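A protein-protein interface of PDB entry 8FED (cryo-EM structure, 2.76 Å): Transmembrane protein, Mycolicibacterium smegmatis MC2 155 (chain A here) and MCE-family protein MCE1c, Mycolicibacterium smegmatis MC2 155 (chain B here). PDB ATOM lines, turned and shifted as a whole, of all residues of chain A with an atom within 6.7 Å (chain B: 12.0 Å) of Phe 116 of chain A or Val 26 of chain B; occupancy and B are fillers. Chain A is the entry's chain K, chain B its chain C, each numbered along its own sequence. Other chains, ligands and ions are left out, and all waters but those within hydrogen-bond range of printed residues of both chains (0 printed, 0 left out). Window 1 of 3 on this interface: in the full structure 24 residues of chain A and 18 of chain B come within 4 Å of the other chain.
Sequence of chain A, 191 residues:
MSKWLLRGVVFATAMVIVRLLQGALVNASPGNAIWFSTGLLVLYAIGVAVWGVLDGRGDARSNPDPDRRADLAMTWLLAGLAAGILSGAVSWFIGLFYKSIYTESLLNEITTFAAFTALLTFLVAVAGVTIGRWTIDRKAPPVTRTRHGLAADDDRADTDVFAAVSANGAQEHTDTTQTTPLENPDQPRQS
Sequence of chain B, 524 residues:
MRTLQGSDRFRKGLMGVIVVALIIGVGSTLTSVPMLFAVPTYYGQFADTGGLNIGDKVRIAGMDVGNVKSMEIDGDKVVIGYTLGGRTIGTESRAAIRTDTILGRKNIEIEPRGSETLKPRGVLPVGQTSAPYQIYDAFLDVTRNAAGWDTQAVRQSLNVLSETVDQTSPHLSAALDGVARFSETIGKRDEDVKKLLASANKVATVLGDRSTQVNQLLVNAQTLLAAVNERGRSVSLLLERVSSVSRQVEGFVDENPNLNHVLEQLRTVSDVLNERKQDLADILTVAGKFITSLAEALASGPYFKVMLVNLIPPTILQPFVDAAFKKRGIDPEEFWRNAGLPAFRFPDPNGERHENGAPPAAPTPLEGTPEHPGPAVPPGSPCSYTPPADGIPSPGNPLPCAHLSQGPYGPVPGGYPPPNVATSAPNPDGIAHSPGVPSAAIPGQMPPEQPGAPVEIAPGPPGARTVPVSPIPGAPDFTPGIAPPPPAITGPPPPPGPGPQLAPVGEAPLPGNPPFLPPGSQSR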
ATOM      1  N   MET A  15      -8.147 -10.253 -23.698  1.00  0.00           N
ATOM      2  CA  MET A  15      -7.545  -9.062 -24.288  1.00  0.00           C
ATOM      3  C   MET A  15      -6.042  -9.019 -24.042  1.00  0.00           C
ATOM      4  O   MET A  15      -5.285  -8.549 -24.897  1.00  0.00           O
ATOM      5  CB  MET A  15      -8.217  -7.805 -23.735  1.00  0.00           C
ATOM      6  CG  MET A  15      -7.982  -6.561 -24.573  1.00  0.00           C
ATOM      7  SD  MET A  15      -8.673  -6.735 -26.227  1.00  0.00           S
ATOM      8  CE  MET A  15      -8.343  -5.118 -26.913  1.00  0.00           C
ATOM      9  N   LEU A  41      -8.438  -8.740 -33.308  1.00  0.00           N
ATOM     10  CA  LEU A  41      -9.611  -8.042 -32.799  1.00  0.00           C
ATOM     11  C   LEU A  41     -10.876  -8.781 -33.201  1.00  0.00           C
ATOM     12  O   LEU A  41     -11.746  -9.047 -32.359  1.00  0.00           O
ATOM     13  CB  LEU A  41      -9.633  -6.601 -33.307  1.00  0.00           C
ATOM     14  CG  LEU A  41      -9.890  -5.525 -32.251  1.00  0.00           C
ATOM     15  CD1 LEU A  41      -8.817  -5.559 -31.173  1.00  0.00           C
ATOM     16  CD2 LEU A  41      -9.965  -4.150 -32.892  1.00  0.00           C
ATOM     17  N   THR A 111      -8.009   4.591 -18.664  1.00  0.00           N
ATOM     18  CA  THR A 111      -9.229   5.278 -19.075  1.00  0.00           C
ATOM     19  C   THR A 111      -9.469   5.246 -20.580  1.00  0.00           C
ATOM     20  O   THR A 111     -10.481   4.707 -21.035  1.00  0.00           O
ATOM     21  CB  THR A 111      -9.195   6.733 -18.585  1.00  0.00           C
ATOM     22  OG1 THR A 111      -8.117   7.428 -19.221  1.00  0.00           O
ATOM     23  CG2 THR A 111      -9.003   6.786 -17.079  1.00  0.00           C
ATOM     24  N   THR A 112      -8.532   5.770 -21.372  1.00  0.00           N
ATOM     25  CA  THR A 112      -8.824   6.097 -22.764  1.00  0.00           C
ATOM     26  C   THR A 112      -8.960   4.848 -23.631  1.00  0.00           C
ATOM     27  O   THR A 112      -9.867   4.763 -24.467  1.00  0.00           O
ATOM     28  CB  THR A 112      -7.729   7.016 -23.302  1.00  0.00           C
ATOM     29  OG1 THR A 112      -7.703   8.226 -22.536  1.00  0.00           O
ATOM     30  CG2 THR A 112      -7.985   7.365 -24.743  1.00  0.00           C
ATOM     31  N   PHE A 113      -8.080   3.867 -23.445  1.00  0.00           N
ATOM     32  CA  PHE A 113      -8.137   2.641 -24.236  1.00  0.00           C
ATOM     33  C   PHE A 113      -9.061   1.602 -23.620  1.00  0.00           C
ATOM     34  O   PHE A 113      -9.639   0.779 -24.347  1.00  0.00           O
ATOM     35  CB  PHE A 113      -6.730   2.068 -24.408  1.00  0.00           C
ATOM     36  CG  PHE A 113      -5.724   3.078 -24.876  1.00  0.00           C
ATOM     37  CD1 PHE A 113      -6.044   3.981 -25.878  1.00  0.00           C
ATOM     38  CD2 PHE A 113      -4.467   3.142 -24.303  1.00  0.00           C
ATOM     39  CE1 PHE A 113      -5.125   4.918 -26.306  1.00  0.00           C
ATOM     40  CE2 PHE A 113      -3.547   4.077 -24.726  1.00  0.00           C
ATOM     41  CZ  PHE A 113      -3.876   4.966 -25.730  1.00  0.00           C
ATOM     42  N   ALA A 114      -9.215   1.627 -22.295  1.00  0.00           N
ATOM     43  CA  ALA A 114     -10.271   0.847 -21.667  1.00  0.00           C
ATOM     44  C   ALA A 114     -11.641   1.284 -22.161  1.00  0.00           C
ATOM     45  O   ALA A 114     -12.557   0.461 -22.239  1.00  0.00           O
ATOM     46  CB  ALA A 114     -10.190   0.967 -20.147  1.00  0.00           C
ATOM     47  N   ALA A 115     -11.798   2.563 -22.515  1.00  0.00           N
ATOM     48  CA  ALA A 115     -13.044   3.009 -23.130  1.00  0.00           C
ATOM     49  C   ALA A 115     -13.284   2.310 -24.463  1.00  0.00           C
ATOM     50  O   ALA A 115     -14.405   1.870 -24.745  1.00  0.00           O
ATOM     51  CB  ALA A 115     -13.025   4.525 -23.316  1.00  0.00           C
ATOM     52  N   PHE A 116     -12.244   2.193 -25.294  1.00  0.00           N
ATOM     53  CA  PHE A 116     -12.379   1.502 -26.574  1.00  0.00           C
ATOM     54  C   PHE A 116     -12.727   0.035 -26.366  1.00  0.00           C
ATOM     55  O   PHE A 116     -13.630  -0.505 -27.021  1.00  0.00           O
ATOM     56  CB  PHE A 116     -11.089   1.645 -27.384  1.00  0.00           C
ATOM     57  CG  PHE A 116     -11.039   0.782 -28.616  1.00  0.00           C
ATOM     58  CD1 PHE A 116     -11.648   1.193 -29.789  1.00  0.00           C
ATOM     59  CD2 PHE A 116     -10.365  -0.430 -28.607  1.00  0.00           C
ATOM     60  CE1 PHE A 116     -11.601   0.407 -30.924  1.00  0.00           C
ATOM     61  CE2 PHE A 116     -10.315  -1.221 -29.738  1.00  0.00           C
ATOM     62  CZ  PHE A 116     -10.933  -0.800 -30.898  1.00  0.00           C
ATOM     63  N   THR A 117     -12.011  -0.625 -25.452  1.00  0.00           N
ATOM     64  CA  THR A 117     -12.272  -2.033 -25.174  1.00  0.00           C
ATOM     65  C   THR A 117     -13.699  -2.235 -24.677  1.00  0.00           C
ATOM     66  O   THR A 117     -14.410  -3.135 -25.139  1.00  0.00           O
ATOM     67  CB  THR A 117     -11.268  -2.560 -24.149  1.00  0.00           C
ATOM     68  OG1 THR A 117      -9.937  -2.402 -24.658  1.00  0.00           O
ATOM     69  CG2 THR A 117     -11.523  -4.029 -23.859  1.00  0.00           C
ATOM     70  N   ALA A 118     -14.138  -1.385 -23.744  1.00  0.00           N
ATOM     71  CA  ALA A 118     -15.473  -1.511 -23.176  1.00  0.00           C
ATOM     72  C   ALA A 118     -16.549  -1.245 -24.217  1.00  0.00           C
ATOM     73  O   ALA A 118     -17.565  -1.944 -24.247  1.00  0.00           O
ATOM     74  CB  ALA A 118     -15.625  -0.560 -21.992  1.00  0.00           C
ATOM     75  N   LEU A 119     -16.356  -0.238 -25.072  1.00  0.00           N
ATOM     76  CA  LEU A 119     -17.354   0.054 -26.097  1.00  0.00           C
ATOM     77  C   LEU A 119     -17.469  -1.090 -27.095  1.00  0.00           C
ATOM     78  O   LEU A 119     -18.582  -1.495 -27.456  1.00  0.00           O
ATOM     79  CB  LEU A 119     -17.017   1.361 -26.814  1.00  0.00           C
ATOM     80  CG  LEU A 119     -18.056   1.805 -27.847  1.00  0.00           C
ATOM     81  CD1 LEU A 119     -19.401   2.034 -27.182  1.00  0.00           C
ATOM     82  CD2 LEU A 119     -17.604   3.053 -28.579  1.00  0.00           C
ATOM     83  N   LEU A 120     -16.333  -1.627 -27.551  1.00  0.00           N
ATOM     84  CA  LEU A 120     -16.373  -2.746 -28.488  1.00  0.00           C
ATOM     85  C   LEU A 120     -17.040  -3.962 -27.858  1.00  0.00           C
ATOM     86  O   LEU A 120     -17.898  -4.607 -28.475  1.00  0.00           O
ATOM     87  CB  LEU A 120     -14.959  -3.091 -28.959  1.00  0.00           C
ATOM     88  CG  LEU A 120     -14.857  -4.208 -29.999  1.00  0.00           C
ATOM     89  CD1 LEU A 120     -15.510  -3.788 -31.304  1.00  0.00           C
ATOM     90  CD2 LEU A 120     -13.409  -4.608 -30.224  1.00  0.00           C
ATOM     91  N   THR A 121     -16.666  -4.277 -26.612  1.00  0.00           N
ATOM     92  CA  THR A 121     -17.260  -5.418 -25.924  1.00  0.00           C
ATOM     93  C   THR A 121     -18.759  -5.225 -25.735  1.00  0.00           C
ATOM     94  O   THR A 121     -19.541  -6.156 -25.947  1.00  0.00           O
ATOM     95  CB  THR A 121     -16.570  -5.634 -24.576  1.00  0.00           C
ATOM     96  OG1 THR A 121     -15.173  -5.870 -24.786  1.00  0.00           O
ATOM     97  CG2 THR A 121     -17.169  -6.827 -23.850  1.00  0.00           C
ATOM     98  N   VAL B  17     -25.250   7.299 -19.973  1.00  0.00           N
ATOM     99  CA  VAL B  17     -24.184   8.281 -19.803  1.00  0.00           C
ATOM    100  C   VAL B  17     -22.820   7.605 -19.912  1.00  0.00           C
ATOM    101  O   VAL B  17     -21.882   8.172 -20.489  1.00  0.00           O
ATOM    102  CB  VAL B  17     -24.353   9.068 -18.486  1.00  0.00           C
ATOM    103  CG1 VAL B  17     -24.083   8.212 -17.255  1.00  0.00           C
ATOM    104  CG2 VAL B  17     -23.466  10.304 -18.489  1.00  0.00           C
ATOM    105  N   ILE B  18     -22.691   6.374 -19.401  1.00  0.00           N
ATOM    106  CA  ILE B  18     -21.433   5.648 -19.557  1.00  0.00           C
ATOM    107  C   ILE B  18     -21.168   5.353 -21.028  1.00  0.00           C
ATOM    108  O   ILE B  18     -20.037   5.505 -21.511  1.00  0.00           O
ATOM    109  CB  ILE B  18     -21.444   4.366 -18.703  1.00  0.00           C
ATOM    110  CG1 ILE B  18     -21.416   4.724 -17.216  1.00  0.00           C
ATOM    111  CG2 ILE B  18     -20.262   3.474 -19.051  1.00  0.00           C
ATOM    112  CD1 ILE B  18     -21.375   3.524 -16.298  1.00  0.00           C
ATOM    113  N   VAL B  19     -22.204   4.951 -21.770  1.00  0.00           N
ATOM    114  CA  VAL B  19     -22.036   4.651 -23.190  1.00  0.00           C
ATOM    115  C   VAL B  19     -21.637   5.902 -23.967  1.00  0.00           C
ATOM    116  O   VAL B  19     -20.757   5.855 -24.833  1.00  0.00           O
ATOM    117  CB  VAL B  19     -23.318   4.010 -23.755  1.00  0.00           C
ATOM    118  CG1 VAL B  19     -23.314   4.039 -25.275  1.00  0.00           C
ATOM    119  CG2 VAL B  19     -23.445   2.580 -23.266  1.00  0.00           C
ATOM    120  N   VAL B  20     -22.272   7.039 -23.670  1.00  0.00           N
ATOM    121  CA  VAL B  20     -21.948   8.275 -24.378  1.00  0.00           C
ATOM    122  C   VAL B  20     -20.526   8.725 -24.061  1.00  0.00           C
ATOM    123  O   VAL B  20     -19.785   9.156 -24.956  1.00  0.00           O
ATOM    124  CB  VAL B  20     -22.983   9.369 -24.053  1.00  0.00           C
ATOM    125  CG1 VAL B  20     -22.541  10.709 -24.616  1.00  0.00           C
ATOM    126  CG2 VAL B  20     -24.335   8.993 -24.627  1.00  0.00           C
ATOM    127  N   ALA B  21     -20.118   8.630 -22.792  1.00  0.00           N
ATOM    128  CA  ALA B  21     -18.743   8.971 -22.436  1.00  0.00           C
ATOM    129  C   ALA B  21     -17.748   8.063 -23.148  1.00  0.00           C
ATOM    130  O   ALA B  21     -16.711   8.527 -23.638  1.00  0.00           O
ATOM    131  CB  ALA B  21     -18.558   8.892 -20.921  1.00  0.00           C
ATOM    132  N   LEU B  22     -18.054   6.763 -23.221  1.00  0.00           N
ATOM    133  CA  LEU B  22     -17.183   5.829 -23.927  1.00  0.00           C
ATOM    134  C   LEU B  22     -17.089   6.169 -25.409  1.00  0.00           C
ATOM    135  O   LEU B  22     -16.001   6.125 -25.993  1.00  0.00           O
ATOM    136  CB  LEU B  22     -17.690   4.399 -23.740  1.00  0.00           C
ATOM    137  CG  LEU B  22     -17.066   3.537 -22.642  1.00  0.00           C
ATOM    138  CD1 LEU B  22     -16.973   4.280 -21.320  1.00  0.00           C
ATOM    139  CD2 LEU B  22     -17.874   2.259 -22.477  1.00  0.00           C
ATOM    140  N   ILE B  23     -18.220   6.504 -26.035  1.00  0.00           N
ATOM    141  CA  ILE B  23     -18.222   6.844 -27.456  1.00  0.00           C
ATOM    142  C   ILE B  23     -17.389   8.095 -27.706  1.00  0.00           C
ATOM    143  O   ILE B  23     -16.610   8.158 -28.666  1.00  0.00           O
ATOM    144  CB  ILE B  23     -19.667   7.007 -27.965  1.00  0.00           C
ATOM    145  CG1 ILE B  23     -20.369   5.649 -28.015  1.00  0.00           C
ATOM    146  CG2 ILE B  23     -19.689   7.662 -29.337  1.00  0.00           C
ATOM    147  CD1 ILE B  23     -21.801   5.720 -28.488  1.00  0.00           C
ATOM    148  N   ILE B  24     -17.539   9.106 -26.847  1.00  0.00           N
ATOM    149  CA  ILE B  24     -16.757  10.332 -26.994  1.00  0.00           C
ATOM    150  C   ILE B  24     -15.270  10.040 -26.832  1.00  0.00           C
ATOM    151  O   ILE B  24     -14.436  10.536 -27.601  1.00  0.00           O
ATOM    152  CB  ILE B  24     -17.246  11.398 -25.995  1.00  0.00           C
ATOM    153  CG1 ILE B  24     -18.667  11.841 -26.346  1.00  0.00           C
ATOM    154  CG2 ILE B  24     -16.304  12.590 -25.970  1.00  0.00           C
ATOM    155  CD1 ILE B  24     -19.232  12.884 -25.411  1.00  0.00           C
ATOM    156  N   GLY B  25     -14.916   9.220 -25.838  1.00  0.00           N
ATOM    157  CA  GLY B  25     -13.517   8.879 -25.636  1.00  0.00           C
ATOM    158  C   GLY B  25     -12.920   8.109 -26.800  1.00  0.00           C
ATOM    159  O   GLY B  25     -11.767   8.332 -27.178  1.00  0.00           O
ATOM    160  N   VAL B  26     -13.690   7.182 -27.376  1.00  0.00           N
ATOM    161  CA  VAL B  26     -13.211   6.427 -28.531  1.00  0.00           C
ATOM    162  C   VAL B  26     -13.037   7.343 -29.736  1.00  0.00           C
ATOM    163  O   VAL B  26     -12.023   7.279 -30.440  1.00  0.00           O
ATOM    164  CB  VAL B  26     -14.163   5.261 -28.848  1.00  0.00           C
ATOM    165  CG1 VAL B  26     -13.757   4.579 -30.145  1.00  0.00           C
ATOM    166  CG2 VAL B  26     -14.150   4.264 -27.719  1.00  0.00           C
ATOM    167  N   GLY B  27     -14.021   8.209 -29.990  1.00  0.00           N
ATOM    168  CA  GLY B  27     -13.905   9.138 -31.101  1.00  0.00           C
ATOM    169  C   GLY B  27     -12.733  10.087 -30.959  1.00  0.00           C
ATOM    170  O   GLY B  27     -12.112  10.465 -31.956  1.00  0.00           O
ATOM    171  N   SER B  28     -12.421  10.490 -29.725  1.00  0.00           N
ATOM    172  CA  SER B  28     -11.299  11.394 -29.495  1.00  0.00           C
ATOM    173  C   SER B  28      -9.971  10.758 -29.889  1.00  0.00           C
ATOM    174  O   SER B  28      -9.112  11.417 -30.486  1.00  0.00           O
ATOM    175  CB  SER B  28     -11.271  11.828 -28.030  1.00  0.00           C
ATOM    176  OG  SER B  28     -12.447  12.538 -27.686  1.00  0.00           O
ATOM    177  N   THR B  29      -9.782   9.482 -29.562  1.00  0.00           N
ATOM    178  CA  THR B  29      -8.515   8.778 -29.757  1.00  0.00           C
ATOM    179  C   THR B  29      -8.716   7.493 -30.549  1.00  0.00           C
ATOM    180  O   THR B  29      -8.217   6.428 -30.183  1.00  0.00           O
ATOM    181  CB  THR B  29      -7.861   8.447 -28.422  1.00  0.00           C
ATOM    182  OG1 THR B  29      -8.721   7.564 -27.693  1.00  0.00           O
ATOM    183  CG2 THR B  29      -7.625   9.709 -27.606  1.00  0.00           C
ATOM    184  N   LEU B  30      -9.465   7.571 -31.650  1.00  0.00           N
ATOM    185  CA  LEU B  30      -9.672   6.379 -32.467  1.00  0.00           C
ATOM    186  C   LEU B  30      -8.391   5.953 -33.175  1.00  0.00           C
ATOM    187  O   LEU B  30      -8.199   4.763 -33.443  1.00  0.00           O
ATOM    188  CB  LEU B  30     -10.790   6.628 -33.480  1.00  0.00           C
ATOM    189  CG  LEU B  30     -11.182   5.470 -34.398  1.00  0.00           C
ATOM    190  CD1 LEU B  30     -11.515   4.231 -33.583  1.00  0.00           C
ATOM    191  CD2 LEU B  30     -12.353   5.864 -35.281  1.00  0.00           C
ATOM    192  N   THR B  31      -7.508   6.901 -33.482  1.00  0.00           N
ATOM    193  CA  THR B  31      -6.265   6.594 -34.178  1.00  0.00           C
ATOM    194  C   THR B  31      -5.125   6.255 -33.225  1.00  0.00           C
ATOM    195  O   THR B  31      -4.202   5.526 -33.604  1.00  0.00           O
ATOM    196  CB  THR B  31      -5.867   7.773 -35.070  1.00  0.00           C
ATOM    197  OG1 THR B  31      -7.020   8.230 -35.782  1.00  0.00           O
ATOM    198  CG2 THR B  31      -4.807   7.360 -36.082  1.00  0.00           C
ATOM    199  N   SER B  32      -5.183   6.743 -31.990  1.00  0.00           N
ATOM    200  CA  SER B  32      -4.106   6.555 -31.028  1.00  0.00           C
ATOM    201  C   SER B  32      -4.210   5.253 -30.243  1.00  0.00           C
ATOM    202  O   SER B  32      -3.345   4.991 -29.401  1.00  0.00           O
ATOM    203  CB  SER B  32      -4.066   7.735 -30.053  1.00  0.00           C
ATOM    204  OG  SER B  32      -3.899   8.960 -30.745  1.00  0.00           O
ATOM    205  N   VAL B  33      -5.235   4.445 -30.482  1.00  0.00           N
ATOM    206  CA  VAL B  33      -5.388   3.199 -29.720  1.00  0.00           C
ATOM    207  C   VAL B  33      -4.294   2.218 -30.134  1.00  0.00           C
ATOM    208  O   VAL B  33      -4.075   2.006 -31.340  1.00  0.00           O
ATOM    209  CB  VAL B  33      -6.789   2.609 -29.931  1.00  0.00           C
ATOM    210  CG1 VAL B  33      -7.134   2.518 -31.408  1.00  0.00           C
ATOM    211  CG2 VAL B  33      -6.899   1.245 -29.272  1.00  0.00           C
ATOM    212  N   PRO B  34      -3.557   1.630 -29.189  1.00  0.00           N
ATOM    213  CA  PRO B  34      -2.475   0.713 -29.569  1.00  0.00           C
ATOM    214  C   PRO B  34      -2.958  -0.660 -30.011  1.00  0.00           C
ATOM    215  O   PRO B  34      -2.276  -1.332 -30.790  1.00  0.00           O
ATOM    216  CB  PRO B  34      -1.637   0.623 -28.288  1.00  0.00           C
ATOM    217  CG  PRO B  34      -2.612   0.875 -27.193  1.00  0.00           C
ATOM    218  CD  PRO B  34      -3.598   1.872 -27.737  1.00  0.00           C
ATOM    219  N   MET B  35      -4.123  -1.098 -29.529  1.00  0.00           N
ATOM    220  CA  MET B  35      -4.610  -2.424 -29.897  1.00  0.00           C
ATOM    221  C   MET B  35      -5.076  -2.505 -31.344  1.00  0.00           C
ATOM    222  O   MET B  35      -5.284  -3.614 -31.845  1.00  0.00           O
ATOM    223  CB  MET B  35      -5.746  -2.857 -28.969  1.00  0.00           C
ATOM    224  CG  MET B  35      -5.351  -2.964 -27.508  1.00  0.00           C
ATOM    225  SD  MET B  35      -5.515  -1.412 -26.609  1.00  0.00           S
ATOM    226  CE  MET B  35      -7.295  -1.228 -26.594  1.00  0.00           C
ATOM    227  N   LEU B  36      -5.244  -1.375 -32.022  1.00  0.00           N
ATOM    228  CA  LEU B  36      -5.701  -1.353 -33.405  1.00  0.00           C
ATOM    229  C   LEU B  36      -4.670  -0.797 -34.372  1.00  0.00           C
ATOM    230  O   LEU B  36      -4.460  -1.376 -35.440  1.00  0.00           O
ATOM    231  CB  LEU B  36      -7.000  -0.541 -33.516  1.00  0.00           C
ATOM    232  CG  LEU B  36      -7.725  -0.593 -34.862  1.00  0.00           C
ATOM    233  CD1 LEU B  36      -8.011  -2.031 -35.256  1.00  0.00           C
ATOM    234  CD2 LEU B  36      -9.014   0.209 -34.804  1.00  0.00           C
ATOM    235  N   PHE B  37      -4.013   0.308 -34.028  1.00  0.00           N
ATOM    236  CA  PHE B  37      -2.990   0.929 -34.869  1.00  0.00           C
ATOM    237  C   PHE B  37      -1.662   0.876 -34.119  1.00  0.00           C
ATOM    238  O   PHE B  37      -1.292   1.824 -33.423  1.00  0.00           O
ATOM    239  CB  PHE B  37      -3.364   2.365 -35.230  1.00  0.00           C
ATOM    240  CG  PHE B  37      -4.691   2.494 -35.916  1.00  0.00           C
ATOM    241  CD1 PHE B  37      -4.811   2.245 -37.272  1.00  0.00           C
ATOM    242  CD2 PHE B  37      -5.818   2.873 -35.207  1.00  0.00           C
ATOM    243  CE1 PHE B  37      -6.032   2.366 -37.907  1.00  0.00           C
ATOM    244  CE2 PHE B  37      -7.040   2.998 -35.837  1.00  0.00           C
ATOM    245  CZ  PHE B  37      -7.147   2.743 -37.188  1.00  0.00           C
ATOM    246  N   ALA B  38      -0.944  -0.234 -34.266  1.00  0.00           N
ATOM    247  CA  ALA B  38       0.347  -0.428 -33.623  1.00  0.00           C
ATOM    248  C   ALA B  38       1.408  -0.666 -34.685  1.00  0.00           C
ATOM    249  O   ALA B  38       1.237  -1.523 -35.559  1.00  0.00           O
ATOM    250  CB  ALA B  38       0.314  -1.603 -32.644  1.00  0.00           C
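OG1 of Thr 111 of chain A sits at hydrogen-bond distance from OG1 of Thr 112 of chain A, at 3.4 Å.
The backbone carbonyl oxygen (O) of Phe 113 of chain A sits at hydrogen-bond distance from the side-chain hydroxyl (OG1) of Thr 117 of chain A, at 3.2 Å.
The backbone carbonyl oxygen of Thr 117 of chain A is in hydrogen-bond range of the side-chain hydroxyl of Thr 121 of chain A (2.9 Å).
O of Gly 25 of chain B is in hydrogen-bond range of OG1 of Thr 29 of chain B (3.2 Å).
Among the printed residues, pairs that only touch across the chains: Thr 112 of chain A with Thr 29 of chain B, Phe 116 of chain A with Val 26 of chain B, Thr 117 of chain A with Met 35 of chain B, Phe 113 of chain A with Ser 32 of chain B, Ala 118 of chain A with Leu 22 of chain B, Phe 113 of chain A with Pro 34 of chain B, Leu 41 of chain A with Leu 36 of chain B, Met 15 of chain A with Met 35 of chain B, Phe 116 of chain A with Met 35 of chain B, Leu 119 of chain A with Val 26 of chain B, Ala 115 of chain A with Leu 22 of chain B, Phe 113 of chain A with Met 35 of chain B, Ala 115 of chain A with Val 26 of chain B, Phe 113 of chain A with Val 33 of chain B, Leu 119 of chain A with Ile 23 of chain B, Phe 116 of chain A with Val 33 of chain B and Leu 119 of chain A with Leu 22 of chain B.
Of chain B, only Val 26 (3.5 Å), Val 33 (3.9 Å) and Met 35 (3.8 Å) come within 4 Å of Phe 116 of chain A.
Val 26 of chain B touches three residues of chain A.
Thr 112 of chain A touches just one residue of chain B: Thr 29.
Ala 115 of chain A touches two residues of chain B.
Of chain B, only Leu 22 (3.6 Å) comes within 4 Å of Ala 118 of chain A.
No residue of chain B comes within 4 Å of Leu 120 of chain A.
Of the printed residues of chain B, Phe 113 of chain A touches Ser 32, Val 33, Pro 34 and Met 35.
Of the printed residues of chain B, Met 15 of chain A touches Met 35 (3.7 Å).
Of the printed residues of chain A, Leu 22 of chain B touches Ala 115, Ala 118 and Leu 119.
Ser 28 of chain B touches none of the printed residues of chain A.
Thr 31 of chain B touches none of the printed residues of chain A.
The nearest residue of chain B that does not touch Phe 116 of chain A is Leu 36 of chain B (4.5 Å).
Of the 13 printed residues of chain A, 9 touch a printed residue of chain B.
Hydrophobic or aromatic side chains of chain A that line the printed part of chain B: Met 15, Leu 41, Phe 113, Phe 116, Ala 118 and Leu 119.
Printed residues of chain B that touch a printed residue of chain A: Leu 22, Ile 23, Val 26, Thr 29, Ser 32, Val 33, Pro 34, Met 35 and Leu 36.
Among the printed residues, no Asp or Glu carboxylate lies within 4 Å of a Lys or Arg side-chain nitrogen of the other chain.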
